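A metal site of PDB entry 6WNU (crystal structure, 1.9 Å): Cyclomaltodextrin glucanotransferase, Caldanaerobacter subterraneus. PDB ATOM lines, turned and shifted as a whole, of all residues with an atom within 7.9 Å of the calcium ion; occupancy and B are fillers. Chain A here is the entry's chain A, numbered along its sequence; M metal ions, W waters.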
ATOM      1  N   PRO A 158      23.666   2.771  17.508  1.00  0.00           N
ATOM      2  CA  PRO A 158      24.352   1.480  17.368  1.00  0.00           C
ATOM      3  C   PRO A 158      24.660   0.792  18.684  1.00  0.00           C
ATOM      4  O   PRO A 158      25.405  -0.191  18.694  1.00  0.00           O
ATOM      5  CB  PRO A 158      25.640   1.871  16.649  1.00  0.00           C
ATOM      6  CG  PRO A 158      25.953   3.225  17.239  1.00  0.00           C
ATOM      7  CD  PRO A 158      24.610   3.898  17.451  1.00  0.00           C
ATOM      8  N   ASN A 159      24.095   1.246  19.799  1.00  0.00           N
ATOM      9  CA  ASN A 159      24.341   0.514  21.021  1.00  0.00           C
ATOM     10  C   ASN A 159      23.518  -0.772  21.113  1.00  0.00           C
ATOM     11  O   ASN A 159      23.906  -1.701  21.826  1.00  0.00           O
ATOM     12  CB  ASN A 159      24.036   1.401  22.235  1.00  0.00           C
ATOM     13  CG  ASN A 159      24.259   0.683  23.541  1.00  0.00           C
ATOM     14  OD1 ASN A 159      25.392   0.349  23.881  1.00  0.00           O
ATOM     15  ND2 ASN A 159      23.185   0.456  24.281  1.00  0.00           N
ATOM     16  N   HIS A 160      22.399  -0.844  20.394  1.00  0.00           N
ATOM     17  CA  HIS A 160      21.434  -1.904  20.668  1.00  0.00           C
ATOM     18  C   HIS A 160      20.460  -2.003  19.504  1.00  0.00           C
ATOM     19  O   HIS A 160      20.396  -1.114  18.642  1.00  0.00           O
ATOM     20  CB  HIS A 160      20.688  -1.635  21.979  1.00  0.00           C
ATOM     21  CG  HIS A 160      20.044  -0.278  22.024  1.00  0.00           C
ATOM     22  ND1 HIS A 160      20.643   0.802  22.628  1.00  0.00           N
ATOM     23  CD2 HIS A 160      18.868   0.179  21.518  1.00  0.00           C
ATOM     24  CE1 HIS A 160      19.873   1.877  22.498  1.00  0.00           C
ATOM     25  NE2 HIS A 160      18.793   1.515  21.815  1.00  0.00           N
ATOM     26  N   HIS A 196      25.636  -8.921  23.826  1.00  0.00           N
ATOM     27  CA  HIS A 196      26.072  -9.206  25.186  1.00  0.00           C
ATOM     28  C   HIS A 196      24.950  -9.923  25.929  1.00  0.00           C
ATOM     29  O   HIS A 196      23.796  -9.489  25.913  1.00  0.00           O
ATOM     30  CB  HIS A 196      26.441  -7.909  25.915  1.00  0.00           C
ATOM     31  CG  HIS A 196      27.693  -7.267  25.416  1.00  0.00           C
ATOM     32  ND1 HIS A 196      27.730  -5.954  24.994  1.00  0.00           N
ATOM     33  CD2 HIS A 196      28.951  -7.746  25.270  1.00  0.00           C
ATOM     34  CE1 HIS A 196      28.961  -5.656  24.595  1.00  0.00           C
ATOM     35  NE2 HIS A 196      29.721  -6.731  24.748  1.00  0.00           N
ATOM     36  N   ILE A 201      21.739  -3.265  33.045  1.00  0.00           N
ATOM     37  CA  ILE A 201      22.555  -2.346  33.835  1.00  0.00           C
ATOM     38  C   ILE A 201      21.935  -2.167  35.218  1.00  0.00           C
ATOM     39  O   ILE A 201      20.719  -1.968  35.357  1.00  0.00           O
ATOM     40  CB  ILE A 201      22.709  -1.000  33.115  1.00  0.00           C
ATOM     41  CG1 ILE A 201      23.479  -1.184  31.822  1.00  0.00           C
ATOM     42  CG2 ILE A 201      23.438   0.021  34.011  1.00  0.00           C
ATOM     43  CD1 ILE A 201      23.564   0.067  30.979  1.00  0.00           C
ATOM     44  N   LYS A 208      32.227  -0.100  32.911  1.00  0.00           N
ATOM     45  CA  LYS A 208      32.165  -1.401  32.235  1.00  0.00           C
ATOM     46  C   LYS A 208      30.762  -1.966  32.275  1.00  0.00           C
ATOM     47  O   LYS A 208      30.310  -2.593  31.307  1.00  0.00           O
ATOM     48  CB  LYS A 208      33.146  -2.383  32.870  1.00  0.00           C
ATOM     49  CG  LYS A 208      34.521  -2.428  32.212  1.00  0.00           C
ATOM     50  CD  LYS A 208      34.530  -3.338  30.991  1.00  0.00           C
ATOM     51  CE  LYS A 208      35.760  -3.082  30.114  1.00  0.00           C
ATOM     52  NZ  LYS A 208      36.644  -1.992  30.626  1.00  0.00           N
ATOM     53  N   GLU A 209      30.052  -1.780  33.381  1.00  0.00           N
ATOM     54  CA  GLU A 209      28.664  -2.214  33.452  1.00  0.00           C
ATOM     55  C   GLU A 209      27.792  -1.401  32.494  1.00  0.00           C
ATOM     56  O   GLU A 209      26.900  -1.945  31.841  1.00  0.00           O
ATOM     57  CB  GLU A 209      28.159  -2.122  34.897  1.00  0.00           C
ATOM     58  CG  GLU A 209      26.688  -2.442  35.050  1.00  0.00           C
ATOM     59  CD  GLU A 209      26.375  -3.203  36.331  1.00  0.00           C
ATOM     60  OE1 GLU A 209      25.216  -3.120  36.798  1.00  0.00           O
ATOM     61  OE2 GLU A 209      27.281  -3.872  36.867  1.00  0.00           O
ATOM     62  N   LEU A 210      28.077  -0.096  32.353  1.00  0.00           N
ATOM     63  CA  LEU A 210      27.320   0.736  31.423  1.00  0.00           C
ATOM     64  C   LEU A 210      27.534   0.315  29.975  1.00  0.00           C
ATOM     65  O   LEU A 210      26.648   0.517  29.135  1.00  0.00           O
ATOM     66  CB  LEU A 210      27.711   2.212  31.558  1.00  0.00           C
ATOM     67  CG  LEU A 210      27.205   2.980  32.770  1.00  0.00           C
ATOM     68  CD1 LEU A 210      27.772   4.381  32.695  1.00  0.00           C
ATOM     69  CD2 LEU A 210      25.700   3.011  32.788  1.00  0.00           C
ATOM     70  N   GLN A 211      28.704  -0.251  29.665  1.00  0.00           N
ATOM     71  CA  GLN A 211      29.039  -0.603  28.306  1.00  0.00           C
ATOM     72  C   GLN A 211      28.673  -2.034  27.939  1.00  0.00           C
ATOM     73  O   GLN A 211      28.314  -2.300  26.782  1.00  0.00           O
ATOM     74  CB  GLN A 211      30.536  -0.418  28.065  1.00  0.00           C
ATOM     75  CG  GLN A 211      31.033   0.995  28.290  1.00  0.00           C
ATOM     76  CD  GLN A 211      32.544   1.078  28.308  1.00  0.00           C
ATOM     77  OE1 GLN A 211      33.231   0.067  28.127  1.00  0.00           O
ATOM     78  NE2 GLN A 211      33.084   2.275  28.511  1.00  0.00           N
ATOM     79  N   ASP A 212      28.732  -2.963  28.893  1.00  0.00           N
ATOM     80  CA  ASP A 212      28.636  -4.383  28.603  1.00  0.00           C
ATOM     81  C   ASP A 212      27.295  -5.009  28.968  1.00  0.00           C
ATOM     82  O   ASP A 212      27.040  -6.146  28.568  1.00  0.00           O
ATOM     83  CB  ASP A 212      29.754  -5.139  29.330  1.00  0.00           C
ATOM     84  CG  ASP A 212      31.133  -4.786  28.791  1.00  0.00           C
ATOM     85  OD1 ASP A 212      31.205  -4.152  27.714  1.00  0.00           O
ATOM     86  OD2 ASP A 212      32.146  -5.160  29.441  1.00  0.00           O
ATOM     87  N   LYS A 213      26.458  -4.311  29.732  1.00  0.00           N
ATOM     88  CA  LYS A 213      25.147  -4.836  30.059  1.00  0.00           C
ATOM     89  C   LYS A 213      24.069  -4.163  29.208  1.00  0.00           C
ATOM     90  O   LYS A 213      24.330  -3.230  28.469  1.00  0.00           O
ATOM     91  CB  LYS A 213      24.866  -4.670  31.554  1.00  0.00           C
ATOM     92  CG  LYS A 213      25.836  -5.480  32.422  1.00  0.00           C
ATOM     93  CD  LYS A 213      25.317  -5.602  33.834  1.00  0.00           C
ATOM     94  CE  LYS A 213      26.033  -6.708  34.604  1.00  0.00           C
ATOM     95  NZ  LYS A 213      25.269  -6.975  35.851  1.00  0.00           N
ATOM     96  N   ASN A 214      22.840  -4.682  29.313  1.00  0.00           N
ATOM     97  CA  ASN A 214      21.730  -4.141  28.549  1.00  0.00           C
ATOM     98  C   ASN A 214      21.256  -2.814  29.122  1.00  0.00           C
ATOM     99  O   ASN A 214      21.083  -2.675  30.335  1.00  0.00           O
ATOM    100  CB  ASN A 214      20.547  -5.117  28.539  1.00  0.00           C
ATOM    101  CG  ASN A 214      20.846  -6.396  27.787  1.00  0.00           C
ATOM    102  OD1 ASN A 214      21.754  -6.448  26.961  1.00  0.00           O
ATOM    103  ND2 ASN A 214      20.068  -7.425  28.064  1.00  0.00           N
ATOM    104  N   LEU A 215      21.043  -1.840  28.246  1.00  0.00           N
ATOM    105  CA  LEU A 215      20.335  -0.614  28.632  1.00  0.00           C
ATOM    106  C   LEU A 215      18.862  -0.957  28.780  1.00  0.00           C
ATOM    107  O   LEU A 215      18.166  -1.148  27.787  1.00  0.00           O
ATOM    108  CB  LEU A 215      20.555   0.464  27.577  1.00  0.00           C
ATOM    109  CG  LEU A 215      19.809   1.790  27.729  1.00  0.00           C
ATOM    110  CD1 LEU A 215      20.011   2.380  29.100  1.00  0.00           C
ATOM    111  CD2 LEU A 215      20.281   2.766  26.654  1.00  0.00           C
ATOM    112  N   LEU A 218      17.086  -3.601  26.397  1.00  0.00           N
ATOM    113  CA  LEU A 218      17.480  -3.459  24.991  1.00  0.00           C
ATOM    114  C   LEU A 218      18.660  -4.388  24.698  1.00  0.00           C
ATOM    115  O   LEU A 218      19.725  -4.260  25.320  1.00  0.00           O
ATOM    116  CB  LEU A 218      17.855  -2.016  24.690  1.00  0.00           C
ATOM    117  CG  LEU A 218      16.753  -0.977  24.904  1.00  0.00           C
ATOM    118  CD1 LEU A 218      17.347   0.431  24.823  1.00  0.00           C
ATOM    119  CD2 LEU A 218      15.624  -1.187  23.874  1.00  0.00           C
ATOM    120  N   ALA A 219      18.474  -5.281  23.734  1.00  0.00           N
ATOM    121  CA  ALA A 219      19.536  -6.234  23.393  1.00  0.00           C
ATOM    122  C   ALA A 219      20.797  -5.500  22.976  1.00  0.00           C
ATOM    123  O   ALA A 219      20.809  -4.774  21.982  1.00  0.00           O
ATOM    124  CB  ALA A 219      19.061  -7.165  22.269  1.00  0.00           C
ATOM    125  N   ASP A 220      21.874  -5.699  23.732  1.00  0.00           N
ATOM    126  CA  ASP A 220      23.065  -4.868  23.627  1.00  0.00           C
ATOM    127  C   ASP A 220      24.039  -5.458  22.608  1.00  0.00           C
ATOM    128  O   ASP A 220      24.475  -6.607  22.769  1.00  0.00           O
ATOM    129  CB  ASP A 220      23.728  -4.754  24.995  1.00  0.00           C
ATOM    130  CG  ASP A 220      24.645  -3.564  25.095  1.00  0.00           C
ATOM    131  OD1 ASP A 220      24.139  -2.425  25.010  1.00  0.00           O
ATOM    132  OD2 ASP A 220      25.866  -3.779  25.249  1.00  0.00           O
ATOM    133  N   LEU A 221      24.406  -4.664  21.601  1.00  0.00           N
ATOM    134  CA  LEU A 221      25.282  -5.156  20.546  1.00  0.00           C
ATOM    135  C   LEU A 221      26.722  -5.207  21.031  1.00  0.00           C
ATOM    136  O   LEU A 221      27.160  -4.334  21.791  1.00  0.00           O
ATOM    137  CB  LEU A 221      25.188  -4.267  19.295  1.00  0.00           C
ATOM    138  CG  LEU A 221      23.903  -4.339  18.447  1.00  0.00           C
ATOM    139  CD1 LEU A 221      23.784  -3.162  17.479  1.00  0.00           C
ATOM    140  CD2 LEU A 221      23.824  -5.663  17.665  1.00  0.00           C
ATOM    141  N   ASP A 222      27.452  -6.219  20.583  1.00  0.00           N
ATOM    142  CA  ASP A 222      28.869  -6.385  20.963  1.00  0.00           C
ATOM    143  C   ASP A 222      29.725  -5.892  19.806  1.00  0.00           C
ATOM    144  O   ASP A 222      30.071  -6.647  18.898  1.00  0.00           O
ATOM    145  CB  ASP A 222      29.179  -7.829  21.315  1.00  0.00           C
ATOM    146  CG  ASP A 222      30.581  -7.996  21.853  1.00  0.00           C
ATOM    147  OD1 ASP A 222      31.293  -6.979  21.995  1.00  0.00           O
ATOM    148  OD2 ASP A 222      30.960  -9.138  22.168  1.00  0.00           O
ATOM    149  N   GLN A 223      30.057  -4.602  19.847  1.00  0.00           N
ATOM    150  CA  GLN A 223      30.892  -4.012  18.817  1.00  0.00           C
ATOM    151  C   GLN A 223      32.288  -4.643  18.754  1.00  0.00           C
ATOM    152  O   GLN A 223      33.007  -4.422  17.774  1.00  0.00           O
ATOM    153  CB  GLN A 223      30.995  -2.486  19.042  1.00  0.00           C
ATOM    154  CG  GLN A 223      29.662  -1.737  19.100  1.00  0.00           C
ATOM    155  CD  GLN A 223      28.982  -1.815  20.457  1.00  0.00           C
ATOM    156  OE1 GLN A 223      29.602  -2.190  21.463  1.00  0.00           O
ATOM    157  NE2 GLN A 223      27.694  -1.468  20.503  1.00  0.00           N
ATOM    158  N   ALA A 251      22.974   7.131  23.080  1.00  0.00           N
ATOM    159  CA  ALA A 251      23.513   6.341  24.193  1.00  0.00           C
ATOM    160  C   ALA A 251      25.030   6.209  24.133  1.00  0.00           C
ATOM    161  O   ALA A 251      25.594   5.127  24.310  1.00  0.00           O
ATOM    162  CB  ALA A 251      22.843   4.962  24.239  1.00  0.00           C
ATOM    163  N   LYS A 253      27.371   6.855  26.118  1.00  0.00           N
ATOM    164  CA  LYS A 253      28.124   6.353  27.276  1.00  0.00           C
ATOM    165  C   LYS A 253      28.026   4.846  27.420  1.00  0.00           C
ATOM    166  O   LYS A 253      28.730   4.261  28.263  1.00  0.00           O
ATOM    167  CB  LYS A 253      27.640   7.049  28.553  1.00  0.00           C
ATOM    168  CG  LYS A 253      26.401   6.444  29.155  1.00  0.00           C
ATOM    169  CD  LYS A 253      25.577   7.462  29.919  1.00  0.00           C
ATOM    170  CE  LYS A 253      26.081   7.703  31.317  1.00  0.00           C
ATOM    171  NZ  LYS A 253      24.957   8.175  32.190  1.00  0.00           N
ATOM    172  N   HIS A 254      27.193   4.192  26.626  1.00  0.00           N
ATOM    173  CA  HIS A 254      26.954   2.761  26.777  1.00  0.00           C
ATOM    174  C   HIS A 254      27.783   1.917  25.829  1.00  0.00           C
ATOM    175  O   HIS A 254      27.616   0.698  25.806  1.00  0.00           O
ATOM    176  CB  HIS A 254      25.477   2.500  26.617  1.00  0.00           C
ATOM    177  CG  HIS A 254      24.681   3.075  27.734  1.00  0.00           C
ATOM    178  ND1 HIS A 254      24.647   2.496  28.979  1.00  0.00           N
ATOM    179  CD2 HIS A 254      23.958   4.216  27.820  1.00  0.00           C
ATOM    180  CE1 HIS A 254      23.899   3.230  29.783  1.00  0.00           C
ATOM    181  NE2 HIS A 254      23.475   4.281  29.101  1.00  0.00           N
ATOM    182  N   MET A 255      28.683   2.538  25.083  1.00  0.00           N
ATOM    183  CA  MET A 255      29.588   1.850  24.201  1.00  0.00           C
ATOM    184  C   MET A 255      31.021   2.153  24.609  1.00  0.00           C
ATOM    185  O   MET A 255      31.290   3.213  25.199  1.00  0.00           O
ATOM    186  CB  MET A 255      29.357   2.292  22.750  1.00  0.00           C
ATOM    187  CG  MET A 255      27.985   1.816  22.225  1.00  0.00           C
ATOM    188  SD  MET A 255      27.541   2.551  20.642  1.00  0.00           S
ATOM    189  CE  MET A 255      26.992   4.189  21.148  1.00  0.00           C
ATOM    190  N   PRO A 256      31.968   1.255  24.327  1.00  0.00           N
ATOM    191  CA  PRO A 256      33.378   1.524  24.663  1.00  0.00           C
ATOM    192  C   PRO A 256      33.899   2.732  23.891  1.00  0.00           C
ATOM    193  O   PRO A 256      33.681   2.858  22.685  1.00  0.00           O
ATOM    194  CB  PRO A 256      34.104   0.246  24.254  1.00  0.00           C
ATOM    195  CG  PRO A 256      33.046  -0.812  24.232  1.00  0.00           C
ATOM    196  CD  PRO A 256      31.795  -0.093  23.763  1.00  0.00           C
HETATM  197 CA    CA M   1      26.780  -1.417  24.975  1.00  0.00          CA
HETATM  198  O   HOH W   1      25.480  -1.035  26.957  1.00  0.00           O
HETATM  199  O   HOH W   2      26.323  -2.053  22.608  1.00  0.00           O
HETATM  200  O   HOH W   3      28.933  -1.793  23.876  1.00  0.00           O
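A ring nitrogen (ND1) of His 254 sits at hydrogen-bond distance from the backbone carbonyl oxygen (O) of Leu 210, at 2.8 Å.
The backbone NH (N) of Leu 221 sits at hydrogen-bond distance from the backbone carbonyl oxygen (O) of Asn 159 (3.0 Å).
N of Asn 159 sits at hydrogen-bond distance from SD of Met 255 (3.8 Å).
The side-chain amide nitrogen (ND2) of Asn 159 sits at hydrogen-bond distance from a ring nitrogen (ND1) of His 160 (3.1 Å).
O of Asp 220 sits at hydrogen-bond distance from N of His 196 (2.8 Å).
The backbone NH of Asp 220 lies close to the side-chain amide oxygen of Asn 214, 3.3 Å away.
Within 4 Å of the calcium ion: Asn 159, Gln 211, Asp 220 and His 254.
Along chain A the residues within 4 Å of the calcium ion span positions 159 to 254.
The calcium ion is bound by water W1 (2.4 Å), the backbone carbonyl oxygen (O) of His 254 (2.4 Å), water W3 (2.4 Å), water W2 (2.5 Å), the side-chain amide oxygen (OD1) of Asn 159 (2.5 Å), the backbone carbonyl oxygen (O) of Gln 211 (2.5 Å), the side-chain carboxylate (OD2) of Asp 220 (2.5 Å) and the side-chain carboxylate (OD1) of Asp 220 (2.8 Å).
The calcium ion has eight donor atoms within binding distance.
Water W2 lies within hydrogen-bond range of O of Leu 221, O of Asn 159 and NE2 of Gln 223.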
